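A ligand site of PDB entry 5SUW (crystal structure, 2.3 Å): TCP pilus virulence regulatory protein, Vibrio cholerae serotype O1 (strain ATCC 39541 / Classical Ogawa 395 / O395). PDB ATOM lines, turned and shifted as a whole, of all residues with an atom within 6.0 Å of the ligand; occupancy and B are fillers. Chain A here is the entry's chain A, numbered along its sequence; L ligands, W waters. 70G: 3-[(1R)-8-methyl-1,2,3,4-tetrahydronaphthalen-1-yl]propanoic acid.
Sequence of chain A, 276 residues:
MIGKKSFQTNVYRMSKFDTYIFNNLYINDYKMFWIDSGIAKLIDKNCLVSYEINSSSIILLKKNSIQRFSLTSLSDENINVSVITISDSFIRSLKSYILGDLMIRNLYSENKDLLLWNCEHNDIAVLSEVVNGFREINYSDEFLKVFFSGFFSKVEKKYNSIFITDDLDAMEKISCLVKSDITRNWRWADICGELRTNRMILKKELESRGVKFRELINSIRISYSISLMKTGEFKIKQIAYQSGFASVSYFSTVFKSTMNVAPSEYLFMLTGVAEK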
ATOM      1  N   GLN A   8      18.507 -19.949  -1.890  1.00  0.00           N
ATOM      2  CA  GLN A   8      17.481 -20.694  -1.179  1.00  0.00           C
ATOM      3  C   GLN A   8      16.150 -20.031  -1.494  1.00  0.00           C
ATOM      4  O   GLN A   8      16.042 -18.795  -1.451  1.00  0.00           O
ATOM      5  CB  GLN A   8      17.742 -20.718   0.334  1.00  0.00           C
ATOM      6  CG  GLN A   8      16.841 -21.657   1.139  1.00  0.00           C
ATOM      7  CD  GLN A   8      15.430 -21.119   1.299  1.00  0.00           C
ATOM      8  OE1 GLN A   8      15.226 -19.903   1.455  1.00  0.00           O
ATOM      9  NE2 GLN A   8      14.441 -22.014   1.239  1.00  0.00           N
ATOM     10  N   ASN A  10      11.603 -20.224  -1.730  1.00  0.00           N
ATOM     11  CA  ASN A  10      10.322 -20.709  -1.224  1.00  0.00           C
ATOM     12  C   ASN A  10       9.184 -19.977  -1.925  1.00  0.00           C
ATOM     13  O   ASN A  10       9.340 -18.849  -2.398  1.00  0.00           O
ATOM     14  CB  ASN A  10      10.208 -20.524   0.294  1.00  0.00           C
ATOM     15  CG  ASN A  10      11.204 -21.376   1.059  1.00  0.00           C
ATOM     16  OD1 ASN A  10      12.241 -20.880   1.503  1.00  0.00           O
ATOM     17  ND2 ASN A  10      10.905 -22.659   1.200  1.00  0.00           N
ATOM     18  N   TYR A  12       5.089 -19.112  -1.096  1.00  0.00           N
ATOM     19  CA  TYR A  12       4.006 -19.090  -0.126  1.00  0.00           C
ATOM     20  C   TYR A  12       2.694 -18.703  -0.791  1.00  0.00           C
ATOM     21  O   TYR A  12       2.643 -17.756  -1.577  1.00  0.00           O
ATOM     22  CB  TYR A  12       4.309 -18.117   0.999  1.00  0.00           C
ATOM     23  CG  TYR A  12       5.647 -18.350   1.656  1.00  0.00           C
ATOM     24  CD1 TYR A  12       6.776 -17.709   1.186  1.00  0.00           C
ATOM     25  CD2 TYR A  12       5.770 -19.196   2.743  1.00  0.00           C
ATOM     26  CE1 TYR A  12       8.003 -17.916   1.786  1.00  0.00           C
ATOM     27  CE2 TYR A  12       6.990 -19.400   3.358  1.00  0.00           C
ATOM     28  CZ  TYR A  12       8.095 -18.762   2.871  1.00  0.00           C
ATOM     29  OH  TYR A  12       9.322 -18.969   3.470  1.00  0.00           O
ATOM     30  N   TYR A  20       0.343 -11.289   5.871  1.00  0.00           N
ATOM     31  CA  TYR A  20       1.575 -11.649   6.564  1.00  0.00           C
ATOM     32  C   TYR A  20       2.067 -10.418   7.333  1.00  0.00           C
ATOM     33  O   TYR A  20       2.000  -9.296   6.832  1.00  0.00           O
ATOM     34  CB  TYR A  20       2.615 -12.115   5.548  1.00  0.00           C
ATOM     35  CG  TYR A  20       2.320 -13.454   4.931  1.00  0.00           C
ATOM     36  CD1 TYR A  20       2.023 -14.563   5.716  1.00  0.00           C
ATOM     37  CD2 TYR A  20       2.336 -13.624   3.545  1.00  0.00           C
ATOM     38  CE1 TYR A  20       1.753 -15.800   5.145  1.00  0.00           C
ATOM     39  CE2 TYR A  20       2.073 -14.856   2.963  1.00  0.00           C
ATOM     40  CZ  TYR A  20       1.778 -15.934   3.776  1.00  0.00           C
ATOM     41  OH  TYR A  20       1.495 -17.160   3.203  1.00  0.00           O
ATOM     42  N   PHE A  22       5.286  -9.048   9.896  1.00  0.00           N
ATOM     43  CA  PHE A  22       6.639  -9.307  10.370  1.00  0.00           C
ATOM     44  C   PHE A  22       7.090  -8.193  11.288  1.00  0.00           C
ATOM     45  O   PHE A  22       6.997  -7.010  10.946  1.00  0.00           O
ATOM     46  CB  PHE A  22       7.586  -9.476   9.199  1.00  0.00           C
ATOM     47  CG  PHE A  22       7.087 -10.452   8.169  1.00  0.00           C
ATOM     48  CD1 PHE A  22       6.996 -11.820   8.483  1.00  0.00           C
ATOM     49  CD2 PHE A  22       6.660 -10.007   6.918  1.00  0.00           C
ATOM     50  CE1 PHE A  22       6.519 -12.743   7.544  1.00  0.00           C
ATOM     51  CE2 PHE A  22       6.168 -10.922   5.965  1.00  0.00           C
ATOM     52  CZ  PHE A  22       6.090 -12.294   6.285  1.00  0.00           C
ATOM     53  N   LEU A  25      11.867  -8.821  12.321  1.00  0.00           N
ATOM     54  CA  LEU A  25      12.400  -9.855  11.455  1.00  0.00           C
ATOM     55  C   LEU A  25      13.812  -9.463  11.047  1.00  0.00           C
ATOM     56  O   LEU A  25      14.013  -8.442  10.375  1.00  0.00           O
ATOM     57  CB  LEU A  25      11.519 -10.033  10.227  1.00  0.00           C
ATOM     58  CG  LEU A  25      11.976 -11.059   9.213  1.00  0.00           C
ATOM     59  CD1 LEU A  25      12.028 -12.437   9.829  1.00  0.00           C
ATOM     60  CD2 LEU A  25      11.014 -11.035   8.047  1.00  0.00           C
ATOM     61  N   ILE A  27      17.129 -10.027   8.871  1.00  0.00           N
ATOM     62  CA  ILE A  27      17.433 -10.504   7.526  1.00  0.00           C
ATOM     63  C   ILE A  27      18.837 -11.099   7.573  1.00  0.00           C
ATOM     64  O   ILE A  27      19.843 -10.373   7.632  1.00  0.00           O
ATOM     65  CB  ILE A  27      17.291  -9.380   6.511  1.00  0.00           C
ATOM     66  CG1 ILE A  27      15.872  -8.817   6.605  1.00  0.00           C
ATOM     67  CG2 ILE A  27      17.575  -9.856   5.079  1.00  0.00           C
ATOM     68  CD1 ILE A  27      14.821  -9.877   6.383  1.00  0.00           C
ATOM     69  N   ASN A  28      18.917 -12.418   7.577  1.00  0.00           N
ATOM     70  CA  ASN A  28      20.202 -13.087   7.773  1.00  0.00           C
ATOM     71  C   ASN A  28      21.061 -13.030   6.515  1.00  0.00           C
ATOM     72  O   ASN A  28      22.295 -13.095   6.601  1.00  0.00           O
ATOM     73  CB  ASN A  28      19.974 -14.543   8.153  1.00  0.00           C
ATOM     74  CG  ASN A  28      19.460 -15.356   6.991  1.00  0.00           C
ATOM     75  OD1 ASN A  28      18.293 -15.235   6.597  1.00  0.00           O
ATOM     76  ND2 ASN A  28      20.323 -16.176   6.406  1.00  0.00           N
ATOM     77  N   LYS A  31      17.675 -10.963   0.578  1.00  0.00           N
ATOM     78  CA  LYS A  31      16.433 -11.596   0.183  1.00  0.00           C
ATOM     79  C   LYS A  31      15.695 -10.700  -0.790  1.00  0.00           C
ATOM     80  O   LYS A  31      15.767  -9.475  -0.693  1.00  0.00           O
ATOM     81  CB  LYS A  31      15.537 -11.861   1.402  1.00  0.00           C
ATOM     82  CG  LYS A  31      16.148 -12.847   2.344  1.00  0.00           C
ATOM     83  CD  LYS A  31      15.200 -13.351   3.393  1.00  0.00           C
ATOM     84  CE  LYS A  31      15.919 -14.363   4.242  1.00  0.00           C
ATOM     85  NZ  LYS A  31      14.934 -15.183   4.947  1.00  0.00           N
ATOM     86  N   PHE A  33      11.651 -10.619  -2.880  1.00  0.00           N
ATOM     87  CA  PHE A  33      10.371 -11.291  -3.060  1.00  0.00           C
ATOM     88  C   PHE A  33       9.462 -10.512  -3.997  1.00  0.00           C
ATOM     89  O   PHE A  33       9.616  -9.298  -4.188  1.00  0.00           O
ATOM     90  CB  PHE A  33       9.672 -11.580  -1.717  1.00  0.00           C
ATOM     91  CG  PHE A  33       9.201 -10.364  -0.950  1.00  0.00           C
ATOM     92  CD1 PHE A  33      10.003  -9.793   0.030  1.00  0.00           C
ATOM     93  CD2 PHE A  33       7.933  -9.856  -1.143  1.00  0.00           C
ATOM     94  CE1 PHE A  33       9.559  -8.695   0.784  1.00  0.00           C
ATOM     95  CE2 PHE A  33       7.477  -8.764  -0.399  1.00  0.00           C
ATOM     96  CZ  PHE A  33       8.296  -8.193   0.563  1.00  0.00           C
ATOM     97  N   LEU A  61      15.214  -6.926   0.442  1.00  0.00           N
ATOM     98  CA  LEU A  61      15.471  -6.729   1.862  1.00  0.00           C
ATOM     99  C   LEU A  61      16.968  -6.824   2.085  1.00  0.00           C
ATOM    100  O   LEU A  61      17.601  -7.814   1.692  1.00  0.00           O
ATOM    101  CB  LEU A  61      14.729  -7.764   2.707  1.00  0.00           C
ATOM    102  CG  LEU A  61      13.228  -7.770   2.397  1.00  0.00           C
ATOM    103  CD1 LEU A  61      12.477  -8.959   3.045  1.00  0.00           C
ATOM    104  CD2 LEU A  61      12.618  -6.422   2.783  1.00  0.00           C
ATOM    105  N   PHE A  69       7.089  -4.936   8.659  1.00  0.00           N
ATOM    106  CA  PHE A  69       6.163  -4.612   7.593  1.00  0.00           C
ATOM    107  C   PHE A  69       5.100  -5.699   7.525  1.00  0.00           C
ATOM    108  O   PHE A  69       5.238  -6.786   8.092  1.00  0.00           O
ATOM    109  CB  PHE A  69       6.870  -4.452   6.238  1.00  0.00           C
ATOM    110  CG  PHE A  69       7.439  -5.721   5.682  1.00  0.00           C
ATOM    111  CD1 PHE A  69       8.726  -6.115   6.000  1.00  0.00           C
ATOM    112  CD2 PHE A  69       6.687  -6.503   4.822  1.00  0.00           C
ATOM    113  CE1 PHE A  69       9.242  -7.275   5.471  1.00  0.00           C
ATOM    114  CE2 PHE A  69       7.203  -7.664   4.293  1.00  0.00           C
ATOM    115  CZ  PHE A  69       8.483  -8.055   4.626  1.00  0.00           C
ATOM    116  N   LEU A  71       2.267  -7.500   4.567  1.00  0.00           N
ATOM    117  CA  LEU A  71       1.903  -7.696   3.180  1.00  0.00           C
ATOM    118  C   LEU A  71       0.484  -8.238   3.170  1.00  0.00           C
ATOM    119  O   LEU A  71       0.215  -9.268   3.812  1.00  0.00           O
ATOM    120  CB  LEU A  71       2.864  -8.669   2.506  1.00  0.00           C
ATOM    121  CG  LEU A  71       2.793  -8.789   0.998  1.00  0.00           C
ATOM    122  CD1 LEU A  71       3.289  -7.482   0.409  1.00  0.00           C
ATOM    123  CD2 LEU A  71       3.666  -9.950   0.581  1.00  0.00           C
ATOM    124  N   VAL A  81       3.499 -15.781  -3.309  1.00  0.00           N
ATOM    125  CA  VAL A  81       4.659 -14.955  -3.046  1.00  0.00           C
ATOM    126  C   VAL A  81       5.903 -15.835  -3.136  1.00  0.00           C
ATOM    127  O   VAL A  81       5.996 -16.870  -2.457  1.00  0.00           O
ATOM    128  CB  VAL A  81       4.561 -14.294  -1.668  1.00  0.00           C
ATOM    129  CG1 VAL A  81       5.661 -13.251  -1.516  1.00  0.00           C
ATOM    130  CG2 VAL A  81       3.187 -13.697  -1.487  1.00  0.00           C
ATOM    131  N   VAL A  83      10.021 -16.047  -2.605  1.00  0.00           N
ATOM    132  CA  VAL A  83      11.116 -15.462  -1.838  1.00  0.00           C
ATOM    133  C   VAL A  83      12.415 -16.143  -2.228  1.00  0.00           C
ATOM    134  O   VAL A  83      12.495 -17.383  -2.264  1.00  0.00           O
ATOM    135  CB  VAL A  83      10.887 -15.588  -0.320  1.00  0.00           C
ATOM    136  CG1 VAL A  83      12.006 -14.832   0.447  1.00  0.00           C
ATOM    137  CG2 VAL A  83       9.498 -15.083   0.051  1.00  0.00           C
ATOM    138  N   THR A  85      16.432 -16.250  -1.059  1.00  0.00           N
ATOM    139  CA  THR A  85      17.497 -15.898  -0.136  1.00  0.00           C
ATOM    140  C   THR A  85      18.809 -16.220  -0.809  1.00  0.00           C
ATOM    141  O   THR A  85      19.002 -17.332  -1.305  1.00  0.00           O
ATOM    142  CB  THR A  85      17.347 -16.665   1.183  1.00  0.00           C
ATOM    143  OG1 THR A  85      16.047 -16.407   1.724  1.00  0.00           O
ATOM    144  CG2 THR A  85      18.419 -16.202   2.173  1.00  0.00           C
ATOM    145  N   SER A 223      15.703 -16.088  12.913  1.00  0.00           N
ATOM    146  CA  SER A 223      16.134 -16.313  11.533  1.00  0.00           C
ATOM    147  C   SER A 223      16.988 -17.564  11.427  1.00  0.00           C
ATOM    148  O   SER A 223      16.890 -18.313  10.450  1.00  0.00           O
ATOM    149  CB  SER A 223      16.894 -15.099  10.988  1.00  0.00           C
ATOM    150  OG  SER A 223      15.940 -14.109  10.601  1.00  0.00           O
ATOM    151  N   ILE A 226      14.554 -20.315  11.303  1.00  0.00           N
ATOM    152  CA  ILE A 226      13.863 -20.399  10.019  1.00  0.00           C
ATOM    153  C   ILE A 226      14.771 -21.075   9.003  1.00  0.00           C
ATOM    154  O   ILE A 226      14.349 -21.956   8.245  1.00  0.00           O
ATOM    155  CB  ILE A 226      13.411 -19.003   9.572  1.00  0.00           C
ATOM    156  CG1 ILE A 226      12.149 -18.614  10.335  1.00  0.00           C
ATOM    157  CG2 ILE A 226      13.175 -18.952   8.054  1.00  0.00           C
ATOM    158  CD1 ILE A 226      11.943 -17.122  10.403  1.00  0.00           C
ATOM    159  N   LYS A 230      14.010 -24.718   6.912  1.00  0.00           N
ATOM    160  CA  LYS A 230      14.044 -24.896   5.458  1.00  0.00           C
ATOM    161  C   LYS A 230      14.863 -26.107   5.044  1.00  0.00           C
ATOM    162  O   LYS A 230      14.621 -26.675   3.973  1.00  0.00           O
ATOM    163  CB  LYS A 230      14.589 -23.633   4.784  1.00  0.00           C
ATOM    164  CG  LYS A 230      13.727 -22.390   5.030  1.00  0.00           C
ATOM    165  CD  LYS A 230      14.470 -21.124   4.682  1.00  0.00           C
ATOM    166  CE  LYS A 230      13.533 -19.968   4.306  1.00  0.00           C
ATOM    167  NZ  LYS A 230      14.324 -18.721   4.016  1.00  0.00           N
ATOM    168  N   MET A 259       6.768 -13.539  13.464  1.00  0.00           N
ATOM    169  CA  MET A 259       6.258 -14.053  12.212  1.00  0.00           C
ATOM    170  C   MET A 259       4.740 -14.093  12.171  1.00  0.00           C
ATOM    171  O   MET A 259       4.185 -14.341  11.098  1.00  0.00           O
ATOM    172  CB  MET A 259       6.801 -15.477  11.982  1.00  0.00           C
ATOM    173  CG  MET A 259       8.316 -15.556  11.926  1.00  0.00           C
ATOM    174  SD  MET A 259       8.979 -14.852  10.403  1.00  0.00           S
ATOM    175  CE  MET A 259       8.408 -16.075   9.194  1.00  0.00           C
ATOM    176  N   TYR A 266       4.477 -22.501  10.467  1.00  0.00           N
ATOM    177  CA  TYR A 266       5.436 -22.100   9.442  1.00  0.00           C
ATOM    178  C   TYR A 266       6.144 -23.310   8.851  1.00  0.00           C
ATOM    179  O   TYR A 266       6.339 -23.393   7.631  1.00  0.00           O
ATOM    180  CB  TYR A 266       6.470 -21.116   9.993  1.00  0.00           C
ATOM    181  CG  TYR A 266       7.494 -20.750   8.952  1.00  0.00           C
ATOM    182  CD1 TYR A 266       7.216 -19.771   8.008  1.00  0.00           C
ATOM    183  CD2 TYR A 266       8.727 -21.379   8.904  1.00  0.00           C
ATOM    184  CE1 TYR A 266       8.125 -19.435   7.035  1.00  0.00           C
ATOM    185  CE2 TYR A 266       9.658 -21.044   7.935  1.00  0.00           C
ATOM    186  CZ  TYR A 266       9.341 -20.072   6.999  1.00  0.00           C
ATOM    187  OH  TYR A 266      10.248 -19.722   6.022  1.00  0.00           O
ATOM    188  N   MET A 269       4.122 -24.545   6.127  1.00  0.00           N
ATOM    189  CA  MET A 269       4.099 -23.711   4.922  1.00  0.00           C
ATOM    190  C   MET A 269       5.284 -24.032   4.007  1.00  0.00           C
ATOM    191  O   MET A 269       5.183 -23.879   2.793  1.00  0.00           O
ATOM    192  CB  MET A 269       4.093 -22.220   5.278  1.00  0.00           C
ATOM    193  CG  MET A 269       2.777 -21.721   5.835  1.00  0.00           C
ATOM    194  SD  MET A 269       2.913 -20.200   6.797  1.00  0.00           S
ATOM    195  CE  MET A 269       3.967 -19.177   5.766  1.00  0.00           C
HETATM  196  C10 70G L   1      10.717 -16.096   5.331  1.00  0.00           C
HETATM  197  C11 70G L   1      12.255 -16.179   5.325  1.00  0.00           C
HETATM  198  C14 70G L   1       6.898 -12.605   2.277  1.00  0.00           C
HETATM  199  C15 70G L   1       5.845 -13.460   2.329  1.00  0.00           C
HETATM  200  C01 70G L   1       6.929 -16.047   4.999  1.00  0.00           C
HETATM  201  C02 70G L   1       6.967 -14.807   4.036  1.00  0.00           C
HETATM  202  C03 70G L   1       8.046 -13.915   3.984  1.00  0.00           C
HETATM  203  C04 70G L   1       8.010 -12.812   3.101  1.00  0.00           C
HETATM  204  C05 70G L   1       9.167 -11.784   2.991  1.00  0.00           C
HETATM  205  C06 70G L   1      10.376 -12.030   3.893  1.00  0.00           C
HETATM  206  C07 70G L   1      10.014 -12.895   5.167  1.00  0.00           C
HETATM  207  C08 70G L   1       9.250 -14.131   4.892  1.00  0.00           C
HETATM  208  C09 70G L   1      10.210 -15.121   4.292  1.00  0.00           C
HETATM  209  O12 70G L   1      12.921 -16.042   6.446  1.00  0.00           O
HETATM  210  O13 70G L   1      12.849 -16.332   4.308  1.00  0.00           O
HETATM  211  C16 70G L   1       5.877 -14.600   3.217  1.00  0.00           C
HETATM  212  O   HOH W   1      11.494 -17.881   2.654  1.00  0.00           O
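NZ of Lys 31 lies within salt-bridge range of O13 of the ligand (2.5 Å).
NZ of Lys 230 is in salt-bridge range of O13 of the ligand, at 2.8 Å.
The backbone carbonyl oxygen of Lys 31 sits at hydrogen-bond distance from the backbone NH of Leu 61, 2.8 Å away.
The side-chain amide oxygen of Gln 8 lies within hydrogen-bond range of the side-chain amino group of Lys 230.
N of Phe 22 is in hydrogen-bond range of O of Phe 69, at 2.9 Å.
OH of Tyr 266 lies within hydrogen-bond range of OH of Tyr 12.
The backbone carbonyl oxygen of Tyr 12 sits at hydrogen-bond distance from the backbone NH of Val 81 (2.8 Å).
O of Leu 71 is in hydrogen-bond range of N of Tyr 20 (2.9 Å).
Tyr 12 touches the ligand (CZ to C01, 3.6 Å).
Tyr 20 touches the ligand (CD2 to C16, 3.7 Å).
CZ of Phe 22 touches C03 of the ligand, 3.4 Å away.
Leu 25 touches the ligand.
CD1 of Phe 33 touches C05 of the ligand (3.7 Å).
CD1 of Leu 61 touches C06 of the ligand, at 3.8 Å.
Val 81 touches the ligand (CG1 to C15, 3.9 Å).
Ile 226 touches the ligand (CG2 to O12, 3.3 Å).
Tyr 266 touches the ligand.
Hydrophobic or aromatic side chains within 4 Å of the ligand: Tyr 12, Tyr 20, Phe 22, Leu 25, Phe 33, Leu 61, Val 81 and Ile 226.
11 residues have an atom within 4 Å of the ligand: Tyr 12, Tyr 20, Phe 22, Leu 25, Lys 31, Phe 33, Leu 61, Val 81, Ile 226, Lys 230 and Tyr 266.
Water W1 lies within hydrogen-bond range of the side-chain hydroxyl of Tyr 12 (2.6 Å), an oxygen (O13) of the ligand (2.6 Å), the side-chain amino group of Lys 230 (3.3 Å) and the side-chain amide oxygen of Asn 10 (3.3 Å).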
